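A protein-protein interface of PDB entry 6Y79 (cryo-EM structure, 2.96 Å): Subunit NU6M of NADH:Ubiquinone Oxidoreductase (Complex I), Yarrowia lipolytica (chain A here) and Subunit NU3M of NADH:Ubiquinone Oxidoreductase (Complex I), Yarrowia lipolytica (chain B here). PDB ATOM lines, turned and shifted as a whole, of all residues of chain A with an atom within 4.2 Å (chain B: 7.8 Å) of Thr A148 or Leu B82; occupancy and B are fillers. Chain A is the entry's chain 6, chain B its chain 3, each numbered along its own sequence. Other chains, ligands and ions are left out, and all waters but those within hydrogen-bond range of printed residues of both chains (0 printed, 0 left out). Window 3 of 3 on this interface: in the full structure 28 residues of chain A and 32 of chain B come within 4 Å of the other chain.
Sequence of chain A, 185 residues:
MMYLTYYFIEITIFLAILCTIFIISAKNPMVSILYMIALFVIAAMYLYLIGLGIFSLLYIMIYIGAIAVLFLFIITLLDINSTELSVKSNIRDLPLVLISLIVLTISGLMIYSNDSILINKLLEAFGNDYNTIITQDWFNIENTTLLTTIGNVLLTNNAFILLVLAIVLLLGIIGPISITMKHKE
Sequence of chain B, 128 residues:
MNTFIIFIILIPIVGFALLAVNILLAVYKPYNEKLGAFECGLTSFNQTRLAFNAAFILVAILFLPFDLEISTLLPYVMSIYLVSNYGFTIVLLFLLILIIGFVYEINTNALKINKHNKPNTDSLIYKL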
ATOM      1  N   THR A 144      -4.752 -10.178 -14.349  1.00  0.00           N
ATOM      2  CA  THR A 144      -3.428  -9.602 -14.483  1.00  0.00           C
ATOM      3  C   THR A 144      -2.439 -10.648 -14.010  1.00  0.00           C
ATOM      4  O   THR A 144      -2.201 -10.806 -12.813  1.00  0.00           O
ATOM      5  CB  THR A 144      -3.305  -8.314 -13.685  1.00  0.00           C
ATOM      6  OG1 THR A 144      -4.352  -7.418 -14.064  1.00  0.00           O
ATOM      7  CG2 THR A 144      -1.988  -7.666 -14.004  1.00  0.00           C
ATOM      8  N   THR A 145      -1.886 -11.396 -14.950  1.00  0.00           N
ATOM      9  CA  THR A 145      -0.788 -12.275 -14.611  1.00  0.00           C
ATOM     10  C   THR A 145       0.520 -11.503 -14.728  1.00  0.00           C
ATOM     11  O   THR A 145       0.542 -10.283 -14.894  1.00  0.00           O
ATOM     12  CB  THR A 145      -0.794 -13.521 -15.491  1.00  0.00           C
ATOM     13  OG1 THR A 145      -0.557 -13.156 -16.855  1.00  0.00           O
ATOM     14  CG2 THR A 145      -2.124 -14.230 -15.378  1.00  0.00           C
ATOM     15  N   LEU A 146       1.623 -12.235 -14.655  1.00  0.00           N
ATOM     16  CA  LEU A 146       2.925 -11.612 -14.468  1.00  0.00           C
ATOM     17  C   LEU A 146       3.417 -10.934 -15.742  1.00  0.00           C
ATOM     18  O   LEU A 146       4.075  -9.887 -15.682  1.00  0.00           O
ATOM     19  CB  LEU A 146       3.898 -12.677 -13.981  1.00  0.00           C
ATOM     20  CG  LEU A 146       5.340 -12.348 -13.671  1.00  0.00           C
ATOM     21  CD1 LEU A 146       5.726 -13.082 -12.432  1.00  0.00           C
ATOM     22  CD2 LEU A 146       6.155 -12.836 -14.815  1.00  0.00           C
ATOM     23  N   LEU A 147       3.105 -11.515 -16.901  1.00  0.00           N
ATOM     24  CA  LEU A 147       3.508 -10.924 -18.171  1.00  0.00           C
ATOM     25  C   LEU A 147       2.764  -9.622 -18.443  1.00  0.00           C
ATOM     26  O   LEU A 147       3.319  -8.707 -19.063  1.00  0.00           O
ATOM     27  CB  LEU A 147       3.276 -11.933 -19.292  1.00  0.00           C
ATOM     28  CG  LEU A 147       3.875 -11.635 -20.659  1.00  0.00           C
ATOM     29  CD1 LEU A 147       5.375 -11.516 -20.560  1.00  0.00           C
ATOM     30  CD2 LEU A 147       3.497 -12.729 -21.625  1.00  0.00           C
ATOM     31  N   THR A 148       1.535  -9.506 -17.940  1.00  0.00           N
ATOM     32  CA  THR A 148       0.786  -8.261 -18.049  1.00  0.00           C
ATOM     33  C   THR A 148       1.431  -7.144 -17.240  1.00  0.00           C
ATOM     34  O   THR A 148       1.537  -6.008 -17.714  1.00  0.00           O
ATOM     35  CB  THR A 148      -0.652  -8.488 -17.594  1.00  0.00           C
ATOM     36  OG1 THR A 148      -1.251  -9.501 -18.408  1.00  0.00           O
ATOM     37  CG2 THR A 148      -1.457  -7.212 -17.719  1.00  0.00           C
ATOM     38  N   THR A 149       1.896  -7.444 -16.025  1.00  0.00           N
ATOM     39  CA  THR A 149       2.485  -6.386 -15.218  1.00  0.00           C
ATOM     40  C   THR A 149       3.883  -6.035 -15.709  1.00  0.00           C
ATOM     41  O   THR A 149       4.292  -4.871 -15.610  1.00  0.00           O
ATOM     42  CB  THR A 149       2.502  -6.793 -13.750  1.00  0.00           C
ATOM     43  OG1 THR A 149       1.240  -7.373 -13.423  1.00  0.00           O
ATOM     44  CG2 THR A 149       2.726  -5.559 -12.875  1.00  0.00           C
ATOM     45  N   ILE A 150       4.612  -7.006 -16.274  1.00  0.00           N
ATOM     46  CA  ILE A 150       5.872  -6.681 -16.944  1.00  0.00           C
ATOM     47  C   ILE A 150       5.616  -5.764 -18.133  1.00  0.00           C
ATOM     48  O   ILE A 150       6.338  -4.784 -18.348  1.00  0.00           O
ATOM     49  CB  ILE A 150       6.623  -7.962 -17.358  1.00  0.00           C
ATOM     50  CG1 ILE A 150       7.135  -8.694 -16.125  1.00  0.00           C
ATOM     51  CG2 ILE A 150       7.818  -7.636 -18.219  1.00  0.00           C
ATOM     52  CD1 ILE A 150       7.864  -9.972 -16.443  1.00  0.00           C
ATOM     53  N   GLY A 151       4.547  -6.018 -18.878  1.00  0.00           N
ATOM     54  CA  GLY A 151       4.181  -5.100 -19.935  1.00  0.00           C
ATOM     55  C   GLY A 151       3.612  -3.774 -19.474  1.00  0.00           C
ATOM     56  O   GLY A 151       3.571  -2.841 -20.277  1.00  0.00           O
ATOM     57  N   ASN A 152       3.130  -3.667 -18.241  1.00  0.00           N
ATOM     58  CA  ASN A 152       2.702  -2.355 -17.770  1.00  0.00           C
ATOM     59  C   ASN A 152       3.882  -1.524 -17.317  1.00  0.00           C
ATOM     60  O   ASN A 152       3.921  -0.322 -17.574  1.00  0.00           O
ATOM     61  CB  ASN A 152       1.703  -2.488 -16.613  1.00  0.00           C
ATOM     62  CG  ASN A 152       0.965  -1.187 -16.283  1.00  0.00           C
ATOM     63  OD1 ASN A 152       1.133  -0.161 -16.943  1.00  0.00           O
ATOM     64  ND2 ASN A 152       0.172  -1.218 -15.214  1.00  0.00           N
ATOM     65  N   LEU B  74       6.133  -9.176 -26.785  1.00  0.00           N
ATOM     66  CA  LEU B  74       5.306 -10.142 -26.086  1.00  0.00           C
ATOM     67  C   LEU B  74       4.844  -9.667 -24.706  1.00  0.00           C
ATOM     68  O   LEU B  74       3.721 -10.010 -24.320  1.00  0.00           O
ATOM     69  CB  LEU B  74       6.064 -11.470 -26.008  1.00  0.00           C
ATOM     70  CG  LEU B  74       5.369 -12.726 -25.516  1.00  0.00           C
ATOM     71  CD1 LEU B  74       4.191 -13.054 -26.398  1.00  0.00           C
ATOM     72  CD2 LEU B  74       6.377 -13.838 -25.552  1.00  0.00           C
ATOM     73  N   PRO B  75       5.625  -8.905 -23.918  1.00  0.00           N
ATOM     74  CA  PRO B  75       4.994  -8.224 -22.781  1.00  0.00           C
ATOM     75  C   PRO B  75       4.022  -7.130 -23.177  1.00  0.00           C
ATOM     76  O   PRO B  75       3.075  -6.879 -22.426  1.00  0.00           O
ATOM     77  CB  PRO B  75       6.187  -7.656 -22.007  1.00  0.00           C
ATOM     78  CG  PRO B  75       7.247  -8.581 -22.276  1.00  0.00           C
ATOM     79  CD  PRO B  75       7.089  -8.944 -23.708  1.00  0.00           C
ATOM     80  N   TYR B  76       4.207  -6.469 -24.321  1.00  0.00           N
ATOM     81  CA  TYR B  76       3.305  -5.374 -24.660  1.00  0.00           C
ATOM     82  C   TYR B  76       1.942  -5.877 -25.096  1.00  0.00           C
ATOM     83  O   TYR B  76       0.916  -5.344 -24.664  1.00  0.00           O
ATOM     84  CB  TYR B  76       3.863  -4.489 -25.765  1.00  0.00           C
ATOM     85  CG  TYR B  76       2.841  -3.436 -26.126  1.00  0.00           C
ATOM     86  CD1 TYR B  76       2.421  -2.516 -25.176  1.00  0.00           C
ATOM     87  CD2 TYR B  76       2.271  -3.375 -27.390  1.00  0.00           C
ATOM     88  CE1 TYR B  76       1.482  -1.564 -25.477  1.00  0.00           C
ATOM     89  CE2 TYR B  76       1.328  -2.419 -27.695  1.00  0.00           C
ATOM     90  CZ  TYR B  76       0.941  -1.520 -26.734  1.00  0.00           C
ATOM     91  OH  TYR B  76       0.003  -0.568 -27.021  1.00  0.00           O
ATOM     92  N   VAL B  77       1.903  -6.890 -25.962  1.00  0.00           N
ATOM     93  CA  VAL B  77       0.627  -7.276 -26.554  1.00  0.00           C
ATOM     94  C   VAL B  77      -0.271  -8.010 -25.564  1.00  0.00           C
ATOM     95  O   VAL B  77      -1.435  -8.271 -25.872  1.00  0.00           O
ATOM     96  CB  VAL B  77       0.856  -8.108 -27.827  1.00  0.00           C
ATOM     97  CG1 VAL B  77       1.703  -7.334 -28.800  1.00  0.00           C
ATOM     98  CG2 VAL B  77       1.516  -9.414 -27.491  1.00  0.00           C
ATOM     99  N   MET B  78       0.236  -8.344 -24.379  1.00  0.00           N
ATOM    100  CA  MET B  78      -0.589  -8.804 -23.275  1.00  0.00           C
ATOM    101  C   MET B  78      -1.083  -7.672 -22.390  1.00  0.00           C
ATOM    102  O   MET B  78      -2.092  -7.838 -21.699  1.00  0.00           O
ATOM    103  CB  MET B  78       0.194  -9.797 -22.419  1.00  0.00           C
ATOM    104  CG  MET B  78       0.427 -11.126 -23.090  1.00  0.00           C
ATOM    105  SD  MET B  78      -1.124 -11.929 -23.492  1.00  0.00           S
ATOM    106  CE  MET B  78      -1.765 -12.205 -21.848  1.00  0.00           C
ATOM    107  N   SER B  79      -0.408  -6.528 -22.398  1.00  0.00           N
ATOM    108  CA  SER B  79      -0.762  -5.391 -21.562  1.00  0.00           C
ATOM    109  C   SER B  79      -1.429  -4.274 -22.348  1.00  0.00           C
ATOM    110  O   SER B  79      -1.511  -3.156 -21.851  1.00  0.00           O
ATOM    111  CB  SER B  79       0.483  -4.851 -20.869  1.00  0.00           C
ATOM    112  OG  SER B  79       1.461  -4.490 -21.826  1.00  0.00           O
ATOM    113  N   ILE B  80      -1.950  -4.571 -23.540  1.00  0.00           N
ATOM    114  CA  ILE B  80      -2.285  -3.547 -24.525  1.00  0.00           C
ATOM    115  C   ILE B  80      -3.470  -2.688 -24.089  1.00  0.00           C
ATOM    116  O   ILE B  80      -3.553  -1.510 -24.455  1.00  0.00           O
ATOM    117  CB  ILE B  80      -2.512  -4.239 -25.887  1.00  0.00           C
ATOM    118  CG1 ILE B  80      -2.720  -3.239 -27.019  1.00  0.00           C
ATOM    119  CG2 ILE B  80      -3.648  -5.233 -25.819  1.00  0.00           C
ATOM    120  CD1 ILE B  80      -2.531  -3.832 -28.370  1.00  0.00           C
ATOM    121  N   TYR B  81      -4.373  -3.219 -23.265  1.00  0.00           N
ATOM    122  CA  TYR B  81      -5.504  -2.401 -22.843  1.00  0.00           C
ATOM    123  C   TYR B  81      -5.117  -1.430 -21.744  1.00  0.00           C
ATOM    124  O   TYR B  81      -5.587  -0.289 -21.735  1.00  0.00           O
ATOM    125  CB  TYR B  81      -6.664  -3.264 -22.361  1.00  0.00           C
ATOM    126  CG  TYR B  81      -7.846  -2.421 -21.963  1.00  0.00           C
ATOM    127  CD1 TYR B  81      -8.578  -1.743 -22.920  1.00  0.00           C
ATOM    128  CD2 TYR B  81      -8.211  -2.276 -20.631  1.00  0.00           C
ATOM    129  CE1 TYR B  81      -9.643  -0.959 -22.572  1.00  0.00           C
ATOM    130  CE2 TYR B  81      -9.277  -1.485 -20.273  1.00  0.00           C
ATOM    131  CZ  TYR B  81      -9.989  -0.832 -21.251  1.00  0.00           C
ATOM    132  OH  TYR B  81     -11.054  -0.043 -20.913  1.00  0.00           O
ATOM    133  N   LEU B  82      -4.284  -1.875 -20.803  1.00  0.00           N
ATOM    134  CA  LEU B  82      -3.977  -1.072 -19.627  1.00  0.00           C
ATOM    135  C   LEU B  82      -3.148   0.150 -19.989  1.00  0.00           C
ATOM    136  O   LEU B  82      -3.370   1.241 -19.456  1.00  0.00           O
ATOM    137  CB  LEU B  82      -3.245  -1.919 -18.594  1.00  0.00           C
ATOM    138  CG  LEU B  82      -4.013  -3.099 -18.021  1.00  0.00           C
ATOM    139  CD1 LEU B  82      -3.096  -3.876 -17.126  1.00  0.00           C
ATOM    140  CD2 LEU B  82      -5.231  -2.637 -17.254  1.00  0.00           C
ATOM    141  N   VAL B  83      -2.172  -0.013 -20.877  1.00  0.00           N
ATOM    142  CA  VAL B  83      -1.429   1.141 -21.355  1.00  0.00           C
ATOM    143  C   VAL B  83      -2.053   1.665 -22.652  1.00  0.00           C
ATOM    144  O   VAL B  83      -1.446   1.622 -23.724  1.00  0.00           O
ATOM    145  CB  VAL B  83       0.064   0.754 -21.484  1.00  0.00           C
ATOM    146  CG1 VAL B  83       0.591   0.452 -20.144  1.00  0.00           C
ATOM    147  CG2 VAL B  83       0.291  -0.529 -22.253  1.00  0.00           C
ATOM    148  N   SER B  84      -3.227   2.280 -22.562  1.00  0.00           N
ATOM    149  CA  SER B  84      -3.926   2.683 -23.778  1.00  0.00           C
ATOM    150  C   SER B  84      -3.670   4.161 -24.007  1.00  0.00           C
ATOM    151  O   SER B  84      -3.861   4.956 -23.086  1.00  0.00           O
ATOM    152  CB  SER B  84      -5.434   2.379 -23.690  1.00  0.00           C
ATOM    153  OG  SER B  84      -6.163   3.316 -22.940  1.00  0.00           O
ATOM    154  N   ASN B  85      -3.214   4.496 -25.223  1.00  0.00           N
ATOM    155  CA  ASN B  85      -2.708   5.763 -25.758  1.00  0.00           C
ATOM    156  C   ASN B  85      -1.299   6.136 -25.298  1.00  0.00           C
ATOM    157  O   ASN B  85      -0.657   6.980 -25.926  1.00  0.00           O
ATOM    158  CB  ASN B  85      -3.616   6.954 -25.432  1.00  0.00           C
ATOM    159  CG  ASN B  85      -5.034   6.733 -25.836  1.00  0.00           C
ATOM    160  OD1 ASN B  85      -5.313   6.037 -26.794  1.00  0.00           O
ATOM    161  ND2 ASN B  85      -5.956   7.312 -25.085  1.00  0.00           N
ATOM    162  N   TYR B  86      -0.753   5.479 -24.283  1.00  0.00           N
ATOM    163  CA  TYR B  86       0.561   5.867 -23.774  1.00  0.00           C
ATOM    164  C   TYR B  86       1.611   4.806 -24.053  1.00  0.00           C
ATOM    165  O   TYR B  86       2.643   5.116 -24.652  1.00  0.00           O
ATOM    166  CB  TYR B  86       0.516   6.170 -22.274  1.00  0.00           C
ATOM    167  CG  TYR B  86       1.840   6.660 -21.751  1.00  0.00           C
ATOM    168  CD1 TYR B  86       2.257   7.954 -21.991  1.00  0.00           C
ATOM    169  CD2 TYR B  86       2.681   5.827 -21.026  1.00  0.00           C
ATOM    170  CE1 TYR B  86       3.467   8.403 -21.528  1.00  0.00           C
ATOM    171  CE2 TYR B  86       3.895   6.273 -20.562  1.00  0.00           C
ATOM    172  CZ  TYR B  86       4.279   7.566 -20.818  1.00  0.00           C
ATOM    173  OH  TYR B  86       5.481   8.036 -20.364  1.00  0.00           O
ATOM    174  N   GLY B  87       1.385   3.563 -23.634  1.00  0.00           N
ATOM    175  CA  GLY B  87       2.266   2.477 -24.021  1.00  0.00           C
ATOM    176  C   GLY B  87       2.236   2.187 -25.500  1.00  0.00           C
ATOM    177  O   GLY B  87       3.190   1.612 -26.030  1.00  0.00           O
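Among the printed residues, merely in contact across the chains: Leu A147 with Leu B74 (3.8 Å), Leu A147 with Pro B75 (3.8 Å), Leu A147 with Met B78 (3.8 Å), Thr A148 with Met B78 (3.8 Å), Thr A148 with Ser B79 (3.5 Å), Thr A148 with Leu B82 (3.8 Å), Gly A151 with Pro B75 (3.3 Å), Asn A152 with Ser B79 (3.9 Å) and Asn A152 with Val B83 (3.3 Å).
The backbone carbonyl oxygen (O) of Pro B75 sits at hydrogen-bond distance from the side-chain hydroxyl (OG) of Ser B79, at 2.9 Å.
O of Tyr B76 sits at hydrogen-bond distance from OG of Ser B79 (3.0 Å).
Printed residues of chain B within 4 Å of Leu A147: Leu B74 (3.8 Å), Pro B75 (3.8 Å) and Met B78 (3.8 Å).
Thr A148 touches just these residues of chain B: Met B78 (3.8 Å), Ser B79 (3.5 Å) and Leu B82 (3.8 Å).
Printed residues of chain A within 4 Å of Leu B74: Leu A147 (3.8 Å).
Of the printed residues of chain A, Pro B75 touches Leu A147 and Gly A151.
Of the printed residues of chain A, Met B78 touches Leu A147 and Thr A148.
Of the printed residues of chain A, Ser B79 touches Thr A148, Gly A151 and Asn A152.
Gly B87 touches none of the printed residues of chain A.
The nearest printed residue of chain A that does not touch Leu B82 is Asn A152 (4.6 Å).
The nearest printed residue of chain A that does not touch Pro B75 is Ile A150 (4.1 Å).
Hydrophobic or aromatic side chains of chain A that line the printed part of chain B: Leu A147.
Of the 14 printed residues of chain B, 6 touch a printed residue of chain A.
Printed residues of chain B that touch a printed residue of chain A: Leu B74, Pro B75, Met B78, Ser B79, Leu B82 and Val B83.
Among the printed residues, 10 pairs touch across the chains.
Among the printed residues, no Asp or Glu carboxylate lies within 4 Å of a Lys or Arg side-chain nitrogen of the other chain.
The side-chain hydroxyl (OG) of Ser B79 lies within hydrogen-bond range of the backbone carbonyl oxygen (O) of Gly A151, at 3.1 Å.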
